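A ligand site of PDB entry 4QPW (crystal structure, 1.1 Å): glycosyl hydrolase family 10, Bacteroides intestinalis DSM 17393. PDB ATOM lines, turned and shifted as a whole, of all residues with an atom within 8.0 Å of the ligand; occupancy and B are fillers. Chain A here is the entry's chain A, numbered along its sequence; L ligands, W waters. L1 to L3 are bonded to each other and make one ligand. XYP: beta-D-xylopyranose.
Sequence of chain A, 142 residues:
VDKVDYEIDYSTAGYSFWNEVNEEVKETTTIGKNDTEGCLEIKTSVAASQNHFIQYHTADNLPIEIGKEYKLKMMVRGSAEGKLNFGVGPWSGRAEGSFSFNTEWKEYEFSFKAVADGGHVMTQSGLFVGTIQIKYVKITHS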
ATOM      1  N   TRP A  18     -18.183   3.299  -7.321  1.00  0.00           N
ATOM      2  CA  TRP A  18     -17.459   3.680  -6.095  1.00  0.00           C
ATOM      3  C   TRP A  18     -16.332   2.694  -5.823  1.00  0.00           C
ATOM      4  O   TRP A  18     -16.476   1.469  -5.949  1.00  0.00           O
ATOM      5  CB  TRP A  18     -18.453   3.673  -4.935  1.00  0.00           C
ATOM      6  CG  TRP A  18     -17.844   4.084  -3.610  1.00  0.00           C
ATOM      7  CD1 TRP A  18     -17.857   5.331  -3.073  1.00  0.00           C
ATOM      8  CD2 TRP A  18     -17.190   3.247  -2.655  1.00  0.00           C
ATOM      9  NE1 TRP A  18     -17.206   5.292  -1.833  1.00  0.00           N
ATOM     10  CE2 TRP A  18     -16.775   4.045  -1.560  1.00  0.00           C
ATOM     11  CE3 TRP A  18     -16.848   1.922  -2.621  1.00  0.00           C
ATOM     12  CZ2 TRP A  18     -16.089   3.501  -0.461  1.00  0.00           C
ATOM     13  CZ3 TRP A  18     -16.130   1.409  -1.527  1.00  0.00           C
ATOM     14  CH2 TRP A  18     -15.815   2.225  -0.467  1.00  0.00           C
ATOM     15  N   ASN A  19     -15.204   3.257  -5.352  1.00  0.00           N
ATOM     16  CA  ASN A  19     -14.100   2.456  -4.916  1.00  0.00           C
ATOM     17  C   ASN A  19     -13.248   3.244  -3.942  1.00  0.00           C
ATOM     18  O   ASN A  19     -13.307   4.481  -3.885  1.00  0.00           O
ATOM     19  CB  ASN A  19     -13.303   1.905  -6.039  1.00  0.00           C
ATOM     20  CG  ASN A  19     -12.719   2.960  -6.887  1.00  0.00           C
ATOM     21  OD1 ASN A  19     -11.534   3.373  -6.599  1.00  0.00           O
ATOM     22  ND2 ASN A  19     -13.403   3.552  -7.838  1.00  0.00           N
ATOM     23  N   GLU A  20     -12.481   2.529  -3.108  1.00  0.00           N
ATOM     24  CA  GLU A  20     -11.655   3.195  -2.098  1.00  0.00           C
ATOM     25  C   GLU A  20     -10.410   2.345  -1.903  1.00  0.00           C
ATOM     26  O   GLU A  20     -10.450   1.254  -1.374  1.00  0.00           O
ATOM     27  CB  GLU A  20     -12.370   3.380  -0.818  1.00  0.00           C
ATOM     28  CG  GLU A  20     -11.591   4.167   0.265  1.00  0.00           C
ATOM     29  CD  GLU A  20     -12.491   4.310   1.465  1.00  0.00           C
ATOM     30  OE1 GLU A  20     -12.678   3.401   2.194  1.00  0.00           O
ATOM     31  OE2 GLU A  20     -13.331   5.247   1.536  1.00  0.00           O
ATOM     32  N   ASN A  22      -7.242   2.447   0.293  1.00  0.00           N
ATOM     33  CA  ASN A  22      -6.603   3.090   1.455  1.00  0.00           C
ATOM     34  C   ASN A  22      -5.239   3.645   1.057  1.00  0.00           C
ATOM     35  O   ASN A  22      -4.502   3.144   0.302  1.00  0.00           O
ATOM     36  CB  ASN A  22      -6.441   2.023   2.536  1.00  0.00           C
ATOM     37  CG  ASN A  22      -6.107   2.608   3.892  1.00  0.00           C
ATOM     38  OD1 ASN A  22      -4.910   2.962   4.115  1.00  0.00           O
ATOM     39  ND2 ASN A  22      -7.037   2.802   4.707  1.00  0.00           N
ATOM     40  N   GLN A  50      -4.994  -4.771   5.704  1.00  0.00           N
ATOM     41  CA  GLN A  50      -6.343  -5.283   5.898  1.00  0.00           C
ATOM     42  C   GLN A  50      -6.966  -5.551   4.524  1.00  0.00           C
ATOM     43  O   GLN A  50      -6.814  -4.765   3.596  1.00  0.00           O
ATOM     44  CB  GLN A  50      -7.225  -4.325   6.694  1.00  0.00           C
ATOM     45  CG  GLN A  50      -6.567  -3.802   8.016  1.00  0.00           C
ATOM     46  CD  GLN A  50      -7.544  -3.498   9.135  1.00  0.00           C
ATOM     47  OE1 GLN A  50      -8.579  -4.187   9.322  1.00  0.00           O
ATOM     48  NE2 GLN A  50      -7.270  -2.401   9.875  1.00  0.00           N
ATOM     49  N   ASN A  51      -7.822  -6.554   4.470  1.00  0.00           N
ATOM     50  CA  ASN A  51      -8.493  -6.840   3.169  1.00  0.00           C
ATOM     51  C   ASN A  51      -9.390  -5.700   2.746  1.00  0.00           C
ATOM     52  O   ASN A  51      -9.448  -5.475   1.506  1.00  0.00           O
ATOM     53  CB  ASN A  51      -9.170  -8.174   3.251  1.00  0.00           C
ATOM     54  CG  ASN A  51      -9.321  -8.834   1.859  1.00  0.00           C
ATOM     55  OD1 ASN A  51      -8.416  -9.096   1.081  1.00  0.00           O
ATOM     56  ND2 ASN A  51     -10.612  -9.049   1.530  1.00  0.00           N
ATOM     57  N   HIS A  52     -10.059  -4.982   3.591  1.00  0.00           N
ATOM     58  CA  HIS A  52     -10.923  -3.920   3.125  1.00  0.00           C
ATOM     59  C   HIS A  52     -10.188  -2.703   2.688  1.00  0.00           C
ATOM     60  O   HIS A  52     -10.853  -1.785   2.188  1.00  0.00           O
ATOM     61  CB  HIS A  52     -11.967  -3.559   4.167  1.00  0.00           C
ATOM     62  CG  HIS A  52     -11.477  -2.768   5.369  1.00  0.00           C
ATOM     63  ND1 HIS A  52     -11.514  -1.398   5.496  1.00  0.00           N
ATOM     64  CD2 HIS A  52     -10.890  -3.248   6.469  1.00  0.00           C
ATOM     65  CE1 HIS A  52     -10.962  -1.056   6.692  1.00  0.00           C
ATOM     66  NE2 HIS A  52     -10.616  -2.175   7.278  1.00  0.00           N
ATOM     67  N   PHE A  53      -8.851  -2.645   2.852  1.00  0.00           N
ATOM     68  CA  PHE A  53      -8.151  -1.485   2.376  1.00  0.00           C
ATOM     69  C   PHE A  53      -8.060  -1.378   0.878  1.00  0.00           C
ATOM     70  O   PHE A  53      -7.630  -0.377   0.346  1.00  0.00           O
ATOM     71  CB  PHE A  53      -6.710  -1.548   2.962  1.00  0.00           C
ATOM     72  CG  PHE A  53      -6.590  -0.997   4.370  1.00  0.00           C
ATOM     73  CD1 PHE A  53      -7.583  -0.797   5.163  1.00  0.00           C
ATOM     74  CD2 PHE A  53      -5.288  -0.686   4.832  1.00  0.00           C
ATOM     75  CE1 PHE A  53      -7.408  -0.259   6.506  1.00  0.00           C
ATOM     76  CE2 PHE A  53      -5.112  -0.212   6.173  1.00  0.00           C
ATOM     77  CZ  PHE A  53      -6.114   0.029   6.960  1.00  0.00           C
ATOM     78  N   GLN A  55     -11.052  -1.867  -1.686  1.00  0.00           N
ATOM     79  CA  GLN A  55     -12.505  -2.220  -1.776  1.00  0.00           C
ATOM     80  C   GLN A  55     -13.151  -1.432  -2.861  1.00  0.00           C
ATOM     81  O   GLN A  55     -12.754  -0.281  -3.166  1.00  0.00           O
ATOM     82  CB  GLN A  55     -13.194  -2.038  -0.431  1.00  0.00           C
ATOM     83  CG  GLN A  55     -13.209  -0.594   0.075  1.00  0.00           C
ATOM     84  CD  GLN A  55     -13.945  -0.428   1.366  1.00  0.00           C
ATOM     85  OE1 GLN A  55     -14.873  -1.175   1.700  1.00  0.00           O
ATOM     86  NE2 GLN A  55     -13.504   0.547   2.183  1.00  0.00           N
ATOM     87  N   TYR A  56     -14.136  -2.060  -3.540  1.00  0.00           N
ATOM     88  CA  TYR A  56     -14.665  -1.488  -4.752  1.00  0.00           C
ATOM     89  C   TYR A  56     -16.012  -2.113  -5.030  1.00  0.00           C
ATOM     90  O   TYR A  56     -16.205  -3.326  -4.842  1.00  0.00           O
ATOM     91  CB  TYR A  56     -13.666  -1.689  -5.928  1.00  0.00           C
ATOM     92  CG  TYR A  56     -13.012  -3.031  -6.024  1.00  0.00           C
ATOM     93  CD1 TYR A  56     -11.862  -3.328  -5.241  1.00  0.00           C
ATOM     94  CD2 TYR A  56     -13.486  -4.064  -6.812  1.00  0.00           C
ATOM     95  CE1 TYR A  56     -11.295  -4.565  -5.195  1.00  0.00           C
ATOM     96  CE2 TYR A  56     -12.913  -5.277  -6.826  1.00  0.00           C
ATOM     97  CZ  TYR A  56     -11.819  -5.576  -6.012  1.00  0.00           C
ATOM     98  OH  TYR A  56     -11.233  -6.819  -6.069  1.00  0.00           O
ATOM     99  N   HIS A  57     -16.911  -1.316  -5.559  1.00  0.00           N
ATOM    100  CA  HIS A  57     -18.185  -1.891  -6.040  1.00  0.00           C
ATOM    101  C   HIS A  57     -17.943  -2.442  -7.411  1.00  0.00           C
ATOM    102  O   HIS A  57     -17.346  -1.800  -8.305  1.00  0.00           O
ATOM    103  CB  HIS A  57     -19.276  -0.829  -6.147  1.00  0.00           C
ATOM    104  CG  HIS A  57     -19.719  -0.268  -4.822  1.00  0.00           C
ATOM    105  ND1 HIS A  57     -20.666   0.737  -4.782  1.00  0.00           N
ATOM    106  CD2 HIS A  57     -19.343  -0.561  -3.544  1.00  0.00           C
ATOM    107  CE1 HIS A  57     -20.851   1.057  -3.503  1.00  0.00           C
ATOM    108  NE2 HIS A  57     -20.069   0.319  -2.746  1.00  0.00           N
ATOM    109  N   TRP A  91     -25.184  -0.291   2.128  1.00  0.00           N
ATOM    110  CA  TRP A  91     -24.162  -0.007   3.115  1.00  0.00           C
ATOM    111  C   TRP A  91     -24.556  -0.508   4.563  1.00  0.00           C
ATOM    112  O   TRP A  91     -23.668  -0.870   5.309  1.00  0.00           O
ATOM    113  CB  TRP A  91     -23.898   1.518   3.200  1.00  0.00           C
ATOM    114  CG  TRP A  91     -23.282   2.073   1.950  1.00  0.00           C
ATOM    115  CD1 TRP A  91     -23.856   2.854   1.030  1.00  0.00           C
ATOM    116  CD2 TRP A  91     -21.919   1.922   1.568  1.00  0.00           C
ATOM    117  NE1 TRP A  91     -22.931   3.118   0.027  1.00  0.00           N
ATOM    118  CE2 TRP A  91     -21.756   2.588   0.333  1.00  0.00           C
ATOM    119  CE3 TRP A  91     -20.857   1.308   2.133  1.00  0.00           C
ATOM    120  CZ2 TRP A  91     -20.512   2.688  -0.334  1.00  0.00           C
ATOM    121  CZ3 TRP A  91     -19.639   1.321   1.376  1.00  0.00           C
ATOM    122  CH2 TRP A  91     -19.542   2.035   0.168  1.00  0.00           C
ATOM    123  N   SER A  92     -25.827  -0.624   4.821  1.00  0.00           N
ATOM    124  CA  SER A  92     -26.226  -1.089   6.179  1.00  0.00           C
ATOM    125  C   SER A  92     -25.971  -2.494   6.434  1.00  0.00           C
ATOM    126  O   SER A  92     -25.863  -2.910   7.643  1.00  0.00           O
ATOM    127  CB  SER A  92     -27.723  -0.781   6.351  1.00  0.00           C
ATOM    128  OG  SER A  92     -28.559  -1.458   5.553  1.00  0.00           O
ATOM    129  N   ARG A  94     -25.287  -6.677   4.338  1.00  0.00           N
ATOM    130  CA  ARG A  94     -25.178  -7.486   3.039  1.00  0.00           C
ATOM    131  C   ARG A  94     -25.216  -8.928   3.287  1.00  0.00           C
ATOM    132  O   ARG A  94     -24.824  -9.434   4.370  1.00  0.00           O
ATOM    133  CB  ARG A  94     -23.885  -7.045   2.278  1.00  0.00           C
ATOM    134  CG  ARG A  94     -23.687  -5.563   2.147  1.00  0.00           C
ATOM    135  CD  ARG A  94     -22.653  -5.232   1.083  1.00  0.00           C
ATOM    136  NE  ARG A  94     -22.309  -3.809   0.995  1.00  0.00           N
ATOM    137  CZ  ARG A  94     -21.425  -3.208   1.822  1.00  0.00           C
ATOM    138  NH1 ARG A  94     -20.799  -3.886   2.737  1.00  0.00           N
ATOM    139  NH2 ARG A  94     -21.219  -1.929   1.707  1.00  0.00           N
ATOM    140  N   GLU A  96     -23.008 -12.000   2.582  1.00  0.00           N
ATOM    141  CA  GLU A  96     -21.570 -12.120   2.445  1.00  0.00           C
ATOM    142  C   GLU A  96     -21.060 -13.420   1.994  1.00  0.00           C
ATOM    143  O   GLU A  96     -21.594 -14.502   2.389  1.00  0.00           O
ATOM    144  CB  GLU A  96     -20.911 -11.731   3.800  1.00  0.00           C
ATOM    145  CG  GLU A  96     -21.161 -10.307   4.243  1.00  0.00           C
ATOM    146  CD  GLU A  96     -20.684 -10.078   5.699  1.00  0.00           C
ATOM    147  OE1 GLU A  96     -19.520 -10.386   5.934  1.00  0.00           O
ATOM    148  OE2 GLU A  96     -21.475  -9.664   6.598  1.00  0.00           O
ATOM    149  N   HIS A 120     -25.483  -2.850  -3.577  1.00  0.00           N
ATOM    150  CA  HIS A 120     -24.353  -3.004  -4.505  1.00  0.00           C
ATOM    151  C   HIS A 120     -23.603  -4.264  -4.195  1.00  0.00           C
ATOM    152  O   HIS A 120     -23.907  -4.996  -3.238  1.00  0.00           O
ATOM    153  CB  HIS A 120     -23.464  -1.745  -4.397  1.00  0.00           C
ATOM    154  CG  HIS A 120     -23.149  -1.406  -2.952  1.00  0.00           C
ATOM    155  ND1 HIS A 120     -23.770  -0.364  -2.280  1.00  0.00           N
ATOM    156  CD2 HIS A 120     -22.302  -1.955  -2.069  1.00  0.00           C
ATOM    157  CE1 HIS A 120     -23.262  -0.320  -1.039  1.00  0.00           C
ATOM    158  NE2 HIS A 120     -22.372  -1.233  -0.873  1.00  0.00           N
ATOM    159  N   MET A 122     -20.283  -5.112  -2.979  1.00  0.00           N
ATOM    160  CA  MET A 122     -19.022  -4.677  -2.343  1.00  0.00           C
ATOM    161  C   MET A 122     -18.029  -5.779  -2.526  1.00  0.00           C
ATOM    162  O   MET A 122     -18.293  -6.946  -2.193  1.00  0.00           O
ATOM    163  CB  MET A 122     -19.274  -4.483  -0.843  1.00  0.00           C
ATOM    164  CG  MET A 122     -18.003  -4.218  -0.077  1.00  0.00           C
ATOM    165  SD  MET A 122     -17.011  -2.830  -0.601  1.00  0.00           S
ATOM    166  CE  MET A 122     -17.975  -1.506   0.211  1.00  0.00           C
ATOM    167  N   THR A 123     -16.812  -5.479  -3.004  1.00  0.00           N
ATOM    168  CA  THR A 123     -15.801  -6.482  -3.344  1.00  0.00           C
ATOM    169  C   THR A 123     -14.502  -6.005  -2.696  1.00  0.00           C
ATOM    170  O   THR A 123     -14.147  -4.820  -2.746  1.00  0.00           O
ATOM    171  CB  THR A 123     -15.669  -6.552  -4.856  1.00  0.00           C
ATOM    172  OG1 THR A 123     -17.024  -6.655  -5.435  1.00  0.00           O
ATOM    173  CG2 THR A 123     -14.945  -7.755  -5.289  1.00  0.00           C
ATOM    174  N   GLN A 124     -13.776  -6.913  -2.036  1.00  0.00           N
ATOM    175  CA  GLN A 124     -12.576  -6.586  -1.263  1.00  0.00           C
ATOM    176  C   GLN A 124     -11.461  -7.574  -1.513  1.00  0.00           C
ATOM    177  O   GLN A 124     -11.714  -8.816  -1.498  1.00  0.00           O
ATOM    178  CB  GLN A 124     -12.900  -6.520   0.231  1.00  0.00           C
ATOM    179  CG  GLN A 124     -14.039  -5.572   0.540  1.00  0.00           C
ATOM    180  CD  GLN A 124     -14.332  -5.281   2.018  1.00  0.00           C
ATOM    181  OE1 GLN A 124     -13.923  -6.066   2.858  1.00  0.00           O
ATOM    182  NE2 GLN A 124     -14.888  -4.186   2.344  1.00  0.00           N
HETATM  183  O1  XYP L   1     -23.050   6.809   0.695  1.00  0.00           O
HETATM  184  C1  XYP L   1     -21.930   6.697   1.520  1.00  0.00           C
HETATM  185  C2  XYP L   1     -22.241   5.876   2.767  1.00  0.00           C
HETATM  186  C3  XYP L   1     -20.960   5.787   3.570  1.00  0.00           C
HETATM  187  C4  XYP L   1     -19.924   5.118   2.678  1.00  0.00           C
HETATM  188  C5  XYP L   1     -19.621   6.016   1.516  1.00  0.00           C
HETATM  189  O2  XYP L   1     -23.275   6.374   3.667  1.00  0.00           O
HETATM  190  O3  XYP L   1     -21.109   4.934   4.691  1.00  0.00           O
HETATM  191  O4  XYP L   1     -18.557   5.225   3.365  1.00  0.00           O
HETATM  192  O5  XYP L   1     -20.898   6.080   0.746  1.00  0.00           O
HETATM  193  C1  XYP L   2     -17.796   4.026   3.371  1.00  0.00           C
HETATM  194  C2  XYP L   2     -16.354   4.504   3.686  1.00  0.00           C
HETATM  195  C3  XYP L   2     -15.526   3.249   3.814  1.00  0.00           C
HETATM  196  C4  XYP L   2     -16.136   2.221   4.700  1.00  0.00           C
HETATM  197  C5  XYP L   2     -17.554   1.911   4.269  1.00  0.00           C
HETATM  198  O2  XYP L   2     -15.835   5.383   2.701  1.00  0.00           O
HETATM  199  O3  XYP L   2     -14.174   3.563   4.282  1.00  0.00           O
HETATM  200  O4  XYP L   2     -15.377   0.989   4.591  1.00  0.00           O
HETATM  201  O5  XYP L   2     -18.330   3.126   4.272  1.00  0.00           O
HETATM  202  C1  XYP L   3     -15.700   0.019   5.534  1.00  0.00           C
HETATM  203  C2  XYP L   3     -15.462  -1.336   4.926  1.00  0.00           C
HETATM  204  C3  XYP L   3     -15.688  -2.457   5.927  1.00  0.00           C
HETATM  205  C4  XYP L   3     -14.814  -2.162   7.182  1.00  0.00           C
HETATM  206  C5  XYP L   3     -15.058  -0.769   7.633  1.00  0.00           C
HETATM  207  O2  XYP L   3     -16.364  -1.542   3.837  1.00  0.00           O
HETATM  208  O3  XYP L   3     -15.334  -3.721   5.312  1.00  0.00           O
HETATM  209  O4  XYP L   3     -15.171  -3.140   8.166  1.00  0.00           O
HETATM  210  O5  XYP L   3     -14.738   0.189   6.634  1.00  0.00           O
HETATM  211  O   HOH W   1     -18.287  -5.027   5.187  1.00  0.00           O
HETATM  212  O   HOH W   2     -17.008   7.555   0.055  1.00  0.00           O
HETATM  213  O   HOH W   3     -25.711   5.959   2.432  1.00  0.00           O
HETATM  214  O   HOH W   4     -19.634   5.349   7.215  1.00  0.00           O
HETATM  215  O   HOH W   5     -21.758   2.601   5.884  1.00  0.00           O
HETATM  216  O   HOH W   6     -12.194   1.759   5.464  1.00  0.00           O
HETATM  217  O   HOH W   7     -14.421  -6.155   6.080  1.00  0.00           O
HETATM  218  O   HOH W   8     -19.160  -1.566   3.775  1.00  0.00           O
HETATM  219  O   HOH W   9     -24.275   6.043  -1.297  1.00  0.00           O
HETATM  220  O   HOH W  10     -16.609   8.076   2.546  1.00  0.00           O
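The side-chain amide oxygen (OE1) of Gln 55 sits at hydrogen-bond distance from an oxygen (O2) of XYP L3, at 2.6 Å.
An oxygen (O3) of XYP L3 sits at hydrogen-bond distance from the side-chain amide nitrogen (NE2) of Gln 124, 3.0 Å away.
An oxygen (O3) of XYP L2 is in hydrogen-bond range of the side-chain carboxylate (OE1) of Glu 20.
ND2 of Asn 51 sits at hydrogen-bond distance from O of Gln 124.
The backbone NH of Glu 20 lies within hydrogen-bond range of the backbone carbonyl oxygen of Gln 55, at 2.8 Å.
OE1 of Gln 55 lies within hydrogen-bond range of NE2 of Gln 124 (3.1 Å).
OE1 of Gln 55 sits close to SD of Met 122, 3.6 Å away.
O of Trp 18 sits at hydrogen-bond distance from N of His 57.
Residues that only touch the ligand: His 52 (3.6 Å), Trp 91 (3.6 Å), Trp 18 (3.7 Å) and Met 122 (3.97 Å).
Hydrophobic or aromatic side chains that line the ligand: Trp 18, His 52, Trp 91 and Met 122.
Of the 19 residues printed, 7 come within 4 Å of the ligand.
The nearest printed residue that does not touch the ligand is Arg 94 (5.1 Å).
Water W9 lies within hydrogen-bond range of O1 of XYP L1 (2.5 Å) and NE1 of Trp 91 (3.5 Å).
Water W7 bridges an oxygen (O3) of XYP L3 and the side-chain amide oxygen of Gln 124.
Water W8 bridges an oxygen (O2) of XYP L3 and the guanidinium group of Arg 94.
Water W6 bridges O3 of XYP L2 (2.9 Å) and ND1 of His 52 (3.2 Å).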
